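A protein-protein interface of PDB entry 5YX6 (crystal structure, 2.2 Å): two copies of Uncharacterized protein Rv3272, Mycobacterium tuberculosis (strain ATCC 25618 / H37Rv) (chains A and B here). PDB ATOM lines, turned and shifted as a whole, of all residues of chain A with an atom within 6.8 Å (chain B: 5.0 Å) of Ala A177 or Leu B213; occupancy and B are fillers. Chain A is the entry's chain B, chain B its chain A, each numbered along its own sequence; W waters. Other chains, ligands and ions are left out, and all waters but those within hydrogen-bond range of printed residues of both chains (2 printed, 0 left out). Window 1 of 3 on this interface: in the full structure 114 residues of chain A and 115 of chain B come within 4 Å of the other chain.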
ATOM      1  N   LEU A  26     -32.141 -11.448   1.329  1.00  0.00           N
ATOM      2  CA  LEU A  26     -30.967 -11.083   2.109  1.00  0.00           C
ATOM      3  C   LEU A  26     -29.720 -11.405   1.307  1.00  0.00           C
ATOM      4  O   LEU A  26     -28.798 -10.602   1.260  1.00  0.00           O
ATOM      5  CB  LEU A  26     -30.929 -11.814   3.455  1.00  0.00           C
ATOM      6  CG  LEU A  26     -29.662 -11.597   4.300  1.00  0.00           C
ATOM      7  CD1 LEU A  26     -29.464 -10.126   4.681  1.00  0.00           C
ATOM      8  CD2 LEU A  26     -29.657 -12.485   5.540  1.00  0.00           C
ATOM      9  N   ASP A 146     -39.281 -20.134   8.197  1.00  0.00           N
ATOM     10  CA  ASP A 146     -38.275 -20.200   9.261  1.00  0.00           C
ATOM     11  C   ASP A 146     -38.753 -21.025  10.458  1.00  0.00           C
ATOM     12  O   ASP A 146     -38.116 -21.998  10.864  1.00  0.00           O
ATOM     13  CB  ASP A 146     -37.911 -18.782   9.733  1.00  0.00           C
ATOM     14  CG  ASP A 146     -36.834 -18.773  10.829  1.00  0.00           C
ATOM     15  OD1 ASP A 146     -37.157 -19.093  11.999  1.00  0.00           O
ATOM     16  OD2 ASP A 146     -35.671 -18.407  10.527  1.00  0.00           O
ATOM     17  N   PHE A 171     -36.867 -14.854  16.683  1.00  0.00           N
ATOM     18  CA  PHE A 171     -36.297 -14.124  15.547  1.00  0.00           C
ATOM     19  C   PHE A 171     -35.930 -15.117  14.455  1.00  0.00           C
ATOM     20  O   PHE A 171     -35.858 -16.322  14.688  1.00  0.00           O
ATOM     21  CB  PHE A 171     -35.089 -13.270  15.954  1.00  0.00           C
ATOM     22  CG  PHE A 171     -33.986 -14.039  16.611  1.00  0.00           C
ATOM     23  CD1 PHE A 171     -32.974 -14.610  15.848  1.00  0.00           C
ATOM     24  CD2 PHE A 171     -33.952 -14.188  17.989  1.00  0.00           C
ATOM     25  CE1 PHE A 171     -31.952 -15.319  16.447  1.00  0.00           C
ATOM     26  CE2 PHE A 171     -32.927 -14.894  18.599  1.00  0.00           C
ATOM     27  CZ  PHE A 171     -31.925 -15.461  17.829  1.00  0.00           C
ATOM     28  N   GLN A 172     -35.729 -14.614  13.250  1.00  0.00           N
ATOM     29  CA  GLN A 172     -35.653 -15.494  12.096  1.00  0.00           C
ATOM     30  C   GLN A 172     -34.215 -15.883  11.831  1.00  0.00           C
ATOM     31  O   GLN A 172     -33.625 -15.456  10.839  1.00  0.00           O
ATOM     32  CB  GLN A 172     -36.271 -14.820  10.860  1.00  0.00           C
ATOM     33  CG  GLN A 172     -37.797 -14.737  10.872  1.00  0.00           C
ATOM     34  CD  GLN A 172     -38.348 -13.875  11.991  1.00  0.00           C
ATOM     35  OE1 GLN A 172     -38.191 -12.653  11.990  1.00  0.00           O
ATOM     36  NE2 GLN A 172     -39.006 -14.513  12.958  1.00  0.00           N
ATOM     37  N   LEU A 173     -33.651 -16.706  12.708  1.00  0.00           N
ATOM     38  CA  LEU A 173     -32.234 -17.019  12.588  1.00  0.00           C
ATOM     39  C   LEU A 173     -31.978 -17.965  11.420  1.00  0.00           C
ATOM     40  O   LEU A 173     -30.914 -17.914  10.816  1.00  0.00           O
ATOM     41  CB  LEU A 173     -31.679 -17.621  13.874  1.00  0.00           C
ATOM     42  CG  LEU A 173     -32.099 -19.056  14.153  1.00  0.00           C
ATOM     43  CD1 LEU A 173     -31.025 -19.777  14.925  1.00  0.00           C
ATOM     44  CD2 LEU A 173     -33.405 -19.074  14.904  1.00  0.00           C
ATOM     45  N   VAL A 174     -32.934 -18.840  11.109  1.00  0.00           N
ATOM     46  CA  VAL A 174     -32.726 -19.803  10.033  1.00  0.00           C
ATOM     47  C   VAL A 174     -32.806 -19.105   8.670  1.00  0.00           C
ATOM     48  O   VAL A 174     -32.009 -19.392   7.779  1.00  0.00           O
ATOM     49  CB  VAL A 174     -33.726 -20.959  10.110  1.00  0.00           C
ATOM     50  CG1 VAL A 174     -33.615 -21.845   8.877  1.00  0.00           C
ATOM     51  CG2 VAL A 174     -33.464 -21.780  11.361  1.00  0.00           C
ATOM     52  N   ASP A 175     -33.748 -18.177   8.520  1.00  0.00           N
ATOM     53  CA  ASP A 175     -33.815 -17.313   7.340  1.00  0.00           C
ATOM     54  C   ASP A 175     -32.516 -16.513   7.117  1.00  0.00           C
ATOM     55  O   ASP A 175     -31.921 -16.557   6.039  1.00  0.00           O
ATOM     56  CB  ASP A 175     -34.999 -16.337   7.449  1.00  0.00           C
ATOM     57  CG  ASP A 175     -36.335 -16.952   7.004  1.00  0.00           C
ATOM     58  OD1 ASP A 175     -36.345 -18.067   6.440  1.00  0.00           O
ATOM     59  OD2 ASP A 175     -37.385 -16.297   7.207  1.00  0.00           O
ATOM     60  N   ASN A 176     -32.086 -15.772   8.130  1.00  0.00           N
ATOM     61  CA  ASN A 176     -30.941 -14.883   7.972  1.00  0.00           C
ATOM     62  C   ASN A 176     -29.613 -15.636   7.831  1.00  0.00           C
ATOM     63  O   ASN A 176     -28.751 -15.232   7.055  1.00  0.00           O
ATOM     64  CB  ASN A 176     -30.889 -13.903   9.133  1.00  0.00           C
ATOM     65  CG  ASN A 176     -32.039 -12.906   9.091  1.00  0.00           C
ATOM     66  OD1 ASN A 176     -32.307 -12.300   8.059  1.00  0.00           O
ATOM     67  ND2 ASN A 176     -32.735 -12.748  10.213  1.00  0.00           N
ATOM     68  N   ALA A 177     -29.447 -16.735   8.562  1.00  0.00           N
ATOM     69  CA  ALA A 177     -28.278 -17.583   8.358  1.00  0.00           C
ATOM     70  C   ALA A 177     -28.277 -18.190   6.951  1.00  0.00           C
ATOM     71  O   ALA A 177     -27.227 -18.314   6.328  1.00  0.00           O
ATOM     72  CB  ALA A 177     -28.215 -18.681   9.413  1.00  0.00           C
ATOM     73  N   SER A 178     -29.451 -18.575   6.454  1.00  0.00           N
ATOM     74  CA  SER A 178     -29.544 -19.189   5.128  1.00  0.00           C
ATOM     75  C   SER A 178     -29.176 -18.220   4.016  1.00  0.00           C
ATOM     76  O   SER A 178     -28.523 -18.601   3.053  1.00  0.00           O
ATOM     77  CB  SER A 178     -30.945 -19.734   4.884  1.00  0.00           C
ATOM     78  OG  SER A 178     -31.194 -20.872   5.693  1.00  0.00           O
ATOM     79  N   GLY A 179     -29.595 -16.970   4.152  1.00  0.00           N
ATOM     80  CA  GLY A 179     -29.219 -15.935   3.207  1.00  0.00           C
ATOM     81  C   GLY A 179     -27.715 -15.779   3.061  1.00  0.00           C
ATOM     82  O   GLY A 179     -27.197 -15.696   1.942  1.00  0.00           O
ATOM     83  N   HIS A 180     -27.011 -15.764   4.192  1.00  0.00           N
ATOM     84  CA  HIS A 180     -25.570 -15.601   4.168  1.00  0.00           C
ATOM     85  C   HIS A 180     -24.883 -16.813   3.580  1.00  0.00           C
ATOM     86  O   HIS A 180     -23.870 -16.685   2.904  1.00  0.00           O
ATOM     87  CB  HIS A 180     -25.037 -15.320   5.570  1.00  0.00           C
ATOM     88  CG  HIS A 180     -25.298 -13.923   6.035  1.00  0.00           C
ATOM     89  ND1 HIS A 180     -24.730 -12.824   5.426  1.00  0.00           N
ATOM     90  CD2 HIS A 180     -26.064 -13.444   7.043  1.00  0.00           C
ATOM     91  CE1 HIS A 180     -25.134 -11.727   6.041  1.00  0.00           C
ATOM     92  NE2 HIS A 180     -25.941 -12.076   7.027  1.00  0.00           N
ATOM     93  N   VAL A 181     -25.446 -17.989   3.814  1.00  0.00           N
ATOM     94  CA  VAL A 181     -24.864 -19.198   3.256  1.00  0.00           C
ATOM     95  C   VAL A 181     -25.075 -19.247   1.741  1.00  0.00           C
ATOM     96  O   VAL A 181     -24.175 -19.637   0.999  1.00  0.00           O
ATOM     97  CB  VAL A 181     -25.435 -20.444   3.941  1.00  0.00           C
ATOM     98  CG1 VAL A 181     -25.075 -21.704   3.177  1.00  0.00           C
ATOM     99  CG2 VAL A 181     -24.925 -20.504   5.391  1.00  0.00           C
ATOM    100  N   LEU A 182     -26.254 -18.827   1.286  1.00  0.00           N
ATOM    101  CA  LEU A 182     -26.535 -18.731  -0.148  1.00  0.00           C
ATOM    102  C   LEU A 182     -25.595 -17.732  -0.829  1.00  0.00           C
ATOM    103  O   LEU A 182     -25.017 -18.017  -1.880  1.00  0.00           O
ATOM    104  CB  LEU A 182     -27.994 -18.331  -0.385  1.00  0.00           C
ATOM    105  CG  LEU A 182     -28.444 -18.228  -1.842  1.00  0.00           C
ATOM    106  CD1 LEU A 182     -28.261 -19.556  -2.576  1.00  0.00           C
ATOM    107  CD2 LEU A 182     -29.895 -17.750  -1.930  1.00  0.00           C
ATOM    108  N   VAL A 204     -28.869 -24.647  -1.617  1.00  0.00           N
ATOM    109  CA  VAL A 204     -28.823 -24.433  -0.186  1.00  0.00           C
ATOM    110  C   VAL A 204     -30.205 -24.694   0.375  1.00  0.00           C
ATOM    111  O   VAL A 204     -31.178 -24.074  -0.049  1.00  0.00           O
ATOM    112  CB  VAL A 204     -28.375 -23.010   0.176  1.00  0.00           C
ATOM    113  CG1 VAL A 204     -28.502 -22.782   1.679  1.00  0.00           C
ATOM    114  CG2 VAL A 204     -26.936 -22.748  -0.293  1.00  0.00           C
ATOM    115  N   VAL A 209     -28.873 -25.821   6.737  1.00  0.00           N
ATOM    116  CA  VAL A 209     -28.283 -24.736   7.496  1.00  0.00           C
ATOM    117  C   VAL A 209     -28.631 -24.880   8.973  1.00  0.00           C
ATOM    118  O   VAL A 209     -27.763 -24.769   9.847  1.00  0.00           O
ATOM    119  CB  VAL A 209     -28.756 -23.372   6.972  1.00  0.00           C
ATOM    120  CG1 VAL A 209     -28.254 -22.256   7.864  1.00  0.00           C
ATOM    121  CG2 VAL A 209     -28.313 -23.170   5.512  1.00  0.00           C
ATOM    122  N   ALA A 210     -29.895 -25.177   9.251  1.00  0.00           N
ATOM    123  CA  ALA A 210     -30.355 -25.316  10.629  1.00  0.00           C
ATOM    124  C   ALA A 210     -29.641 -26.479  11.318  1.00  0.00           C
ATOM    125  O   ALA A 210     -29.228 -26.366  12.481  1.00  0.00           O
ATOM    126  CB  ALA A 210     -31.868 -25.502  10.680  1.00  0.00           C
ATOM    127  N   LEU A 213     -26.066 -25.272  12.169  1.00  0.00           N
ATOM    128  CA  LEU A 213     -25.998 -24.415  13.351  1.00  0.00           C
ATOM    129  C   LEU A 213     -26.019 -25.218  14.663  1.00  0.00           C
ATOM    130  O   LEU A 213     -25.538 -24.741  15.690  1.00  0.00           O
ATOM    131  CB  LEU A 213     -27.149 -23.408  13.353  1.00  0.00           C
ATOM    132  CG  LEU A 213     -27.177 -22.393  12.209  1.00  0.00           C
ATOM    133  CD1 LEU A 213     -28.423 -21.521  12.298  1.00  0.00           C
ATOM    134  CD2 LEU A 213     -25.928 -21.541  12.237  1.00  0.00           C
ATOM    135  N   MET B 155     -30.296 -11.802  22.309  1.00  0.00           N
ATOM    136  CA  MET B 155     -30.932 -13.039  21.861  1.00  0.00           C
ATOM    137  C   MET B 155     -31.736 -13.787  22.927  1.00  0.00           C
ATOM    138  O   MET B 155     -32.306 -14.839  22.635  1.00  0.00           O
ATOM    139  CB  MET B 155     -29.879 -13.980  21.280  1.00  0.00           C
ATOM    140  CG  MET B 155     -29.362 -13.508  19.938  1.00  0.00           C
ATOM    141  SD  MET B 155     -28.162 -14.628  19.208  1.00  0.00           S
ATOM    142  CE  MET B 155     -28.219 -14.074  17.499  1.00  0.00           C
ATOM    143  N   LEU B 173     -25.149 -20.732  17.852  1.00  0.00           N
ATOM    144  CA  LEU B 173     -25.610 -20.189  16.587  1.00  0.00           C
ATOM    145  C   LEU B 173     -24.736 -19.028  16.138  1.00  0.00           C
ATOM    146  O   LEU B 173     -24.530 -18.834  14.944  1.00  0.00           O
ATOM    147  CB  LEU B 173     -27.069 -19.735  16.680  1.00  0.00           C
ATOM    148  CG  LEU B 173     -27.342 -18.455  17.468  1.00  0.00           C
ATOM    149  CD1 LEU B 173     -28.548 -17.723  16.918  1.00  0.00           C
ATOM    150  CD2 LEU B 173     -27.532 -18.773  18.938  1.00  0.00           C
ATOM    151  N   ALA B 177     -22.827 -19.223  12.596  1.00  0.00           N
ATOM    152  CA  ALA B 177     -23.196 -18.171  11.649  1.00  0.00           C
ATOM    153  C   ALA B 177     -22.006 -17.270  11.327  1.00  0.00           C
ATOM    154  O   ALA B 177     -21.822 -16.871  10.175  1.00  0.00           O
ATOM    155  CB  ALA B 177     -24.360 -17.337  12.183  1.00  0.00           C
ATOM    156  N   VAL B 209     -22.748 -10.020  13.505  1.00  0.00           N
ATOM    157  CA  VAL B 209     -23.493 -11.137  12.961  1.00  0.00           C
ATOM    158  C   VAL B 209     -24.753 -11.414  13.779  1.00  0.00           C
ATOM    159  O   VAL B 209     -25.822 -11.643  13.218  1.00  0.00           O
ATOM    160  CB  VAL B 209     -22.630 -12.396  12.897  1.00  0.00           C
ATOM    161  CG1 VAL B 209     -23.463 -13.575  12.396  1.00  0.00           C
ATOM    162  CG2 VAL B 209     -21.416 -12.159  11.983  1.00  0.00           C
ATOM    163  N   ALA B 210     -24.620 -11.383  15.104  1.00  0.00           N
ATOM    164  CA  ALA B 210     -25.732 -11.666  16.003  1.00  0.00           C
ATOM    165  C   ALA B 210     -26.829 -10.622  15.858  1.00  0.00           C
ATOM    166  O   ALA B 210     -28.010 -10.965  15.782  1.00  0.00           O
ATOM    167  CB  ALA B 210     -25.257 -11.725  17.443  1.00  0.00           C
ATOM    168  N   VAL B 211     -26.424  -9.356  15.805  1.00  0.00           N
ATOM    169  CA  VAL B 211     -27.350  -8.256  15.555  1.00  0.00           C
ATOM    170  C   VAL B 211     -28.060  -8.504  14.226  1.00  0.00           C
ATOM    171  O   VAL B 211     -29.280  -8.393  14.128  1.00  0.00           O
ATOM    172  CB  VAL B 211     -26.615  -6.891  15.541  1.00  0.00           C
ATOM    173  CG1 VAL B 211     -27.445  -5.831  14.849  1.00  0.00           C
ATOM    174  CG2 VAL B 211     -26.252  -6.454  16.967  1.00  0.00           C
ATOM    175  N   GLY B 212     -27.284  -8.880  13.215  1.00  0.00           N
ATOM    176  CA  GLY B 212     -27.830  -9.172  11.904  1.00  0.00           C
ATOM    177  C   GLY B 212     -28.876 -10.269  11.906  1.00  0.00           C
ATOM    178  O   GLY B 212     -29.880 -10.163  11.219  1.00  0.00           O
ATOM    179  N   LEU B 213     -28.645 -11.325  12.675  1.00  0.00           N
ATOM    180  CA  LEU B 213     -29.613 -12.416  12.767  1.00  0.00           C
ATOM    181  C   LEU B 213     -30.960 -11.984  13.356  1.00  0.00           C
ATOM    182  O   LEU B 213     -31.976 -12.607  13.079  1.00  0.00           O
ATOM    183  CB  LEU B 213     -29.029 -13.574  13.586  1.00  0.00           C
ATOM    184  CG  LEU B 213     -27.809 -14.265  12.956  1.00  0.00           C
ATOM    185  CD1 LEU B 213     -27.246 -15.316  13.903  1.00  0.00           C
ATOM    186  CD2 LEU B 213     -28.157 -14.900  11.600  1.00  0.00           C
ATOM    187  N   GLN B 214     -30.959 -10.905  14.135  1.00  0.00           N
ATOM    188  CA  GLN B 214     -32.165 -10.400  14.786  1.00  0.00           C
ATOM    189  C   GLN B 214     -32.661  -9.097  14.161  1.00  0.00           C
ATOM    190  O   GLN B 214     -33.424  -8.355  14.779  1.00  0.00           O
ATOM    191  CB  GLN B 214     -31.903 -10.135  16.270  1.00  0.00           C
ATOM    192  CG  GLN B 214     -31.157 -11.201  17.026  1.00  0.00           C
ATOM    193  CD  GLN B 214     -30.676 -10.676  18.366  1.00  0.00           C
ATOM    194  OE1 GLN B 214     -31.404 -10.731  19.363  1.00  0.00           O
ATOM    195  NE2 GLN B 214     -29.450 -10.161  18.402  1.00  0.00           N
ATOM    196  N   ALA B 215     -32.219  -8.819  12.943  1.00  0.00           N
ATOM    197  CA  ALA B 215     -32.390  -7.500  12.327  1.00  0.00           C
ATOM    198  C   ALA B 215     -33.838  -6.999  12.292  1.00  0.00           C
ATOM    199  O   ALA B 215     -34.082  -5.837  12.588  1.00  0.00           O
ATOM    200  CB  ALA B 215     -31.808  -7.512  10.907  1.00  0.00           C
HETATM  201  O   HOH W   1     -26.066 -11.981  10.457  1.00  0.00           O
HETATM  202  O   HOH W   2     -34.864 -12.077  12.619  1.00  0.00           O
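O of Leu B213 sits at hydrogen-bond distance from ND2 of Asn A176 (3.0 Å).
The side-chain carboxylate (OD2) of Asp A146 is in hydrogen-bond range of the backbone NH (N) of Leu A173 (3.4 Å). OE1 of Gln B214 is in hydrogen-bond range of N of Met B155, 3.3 Å away. O of Gln A172 lies within hydrogen-bond range of ND2 of Asn A176 (2.9 Å).
Among the printed residues, merely in contact across the chains: Phe A171 with Met B155 (3.9 Å), Phe A171 with Leu B213 (3.6 Å), Gln A172 with Leu B213 (3.98 Å), Leu A173 with Leu B173 (3.8 Å), Asn A176 with Gly B212 (3.98 Å), Ala A177 with Leu B213 (3.8 Å) and Leu A213 with Ala B177 (3.9 Å).
Ala A177 touches just one residue of chain B: Leu B213 (3.8 Å). Of the printed residues of chain A, Leu B213 touches Phe A171 (3.6 Å), Gln A172 (3.98 Å), Asn A176 (3.0 Å) and Ala A177 (3.8 Å). Of the printed residues of chain B, Phe A171 touches Met B155 (3.9 Å) and Leu B213 (3.6 Å). Of the printed residues of chain A, Ala B177 touches Leu A213. Ala B215 touches none of the printed residues of chain A. The nearest residue of chain B that does not touch Ala A177 is Ala B177 (4.9 Å).
Printed residues of chain A that touch a printed residue of chain B: Phe A171, Gln A172, Leu A173, Asn A176, Ala A177 and Leu A213. Hydrophobic or aromatic side chains of chain A that line the printed part of chain B: Phe A171, Leu A173 and Leu A213. Among the printed residues, no Asp or Glu carboxylate lies within 4 Å of a Lys or Arg side-chain nitrogen of the other chain.
Leu A173 touches its own counterpart, Leu B173. Ala A177 touches Leu B213, and with the chains exchanged Leu A213 touches Ala B177. Positions printed for both chains: 173, 177, 209, 210 and 213.
Water W2 lies within hydrogen-bond range of the backbone NH (N) of Gln A172 (2.8 Å), the backbone carbonyl oxygen (O) of Leu B213 (3.0 Å) and the side-chain amide nitrogen (ND2) of Asn A176 (3.3 Å). Water W1 lies within hydrogen-bond range of the backbone carbonyl oxygen (O) of Val B209 (2.8 Å), a ring nitrogen (NE2) of His A180 (3.4 Å) and the backbone NH (N) of Leu B213 (3.5 Å).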
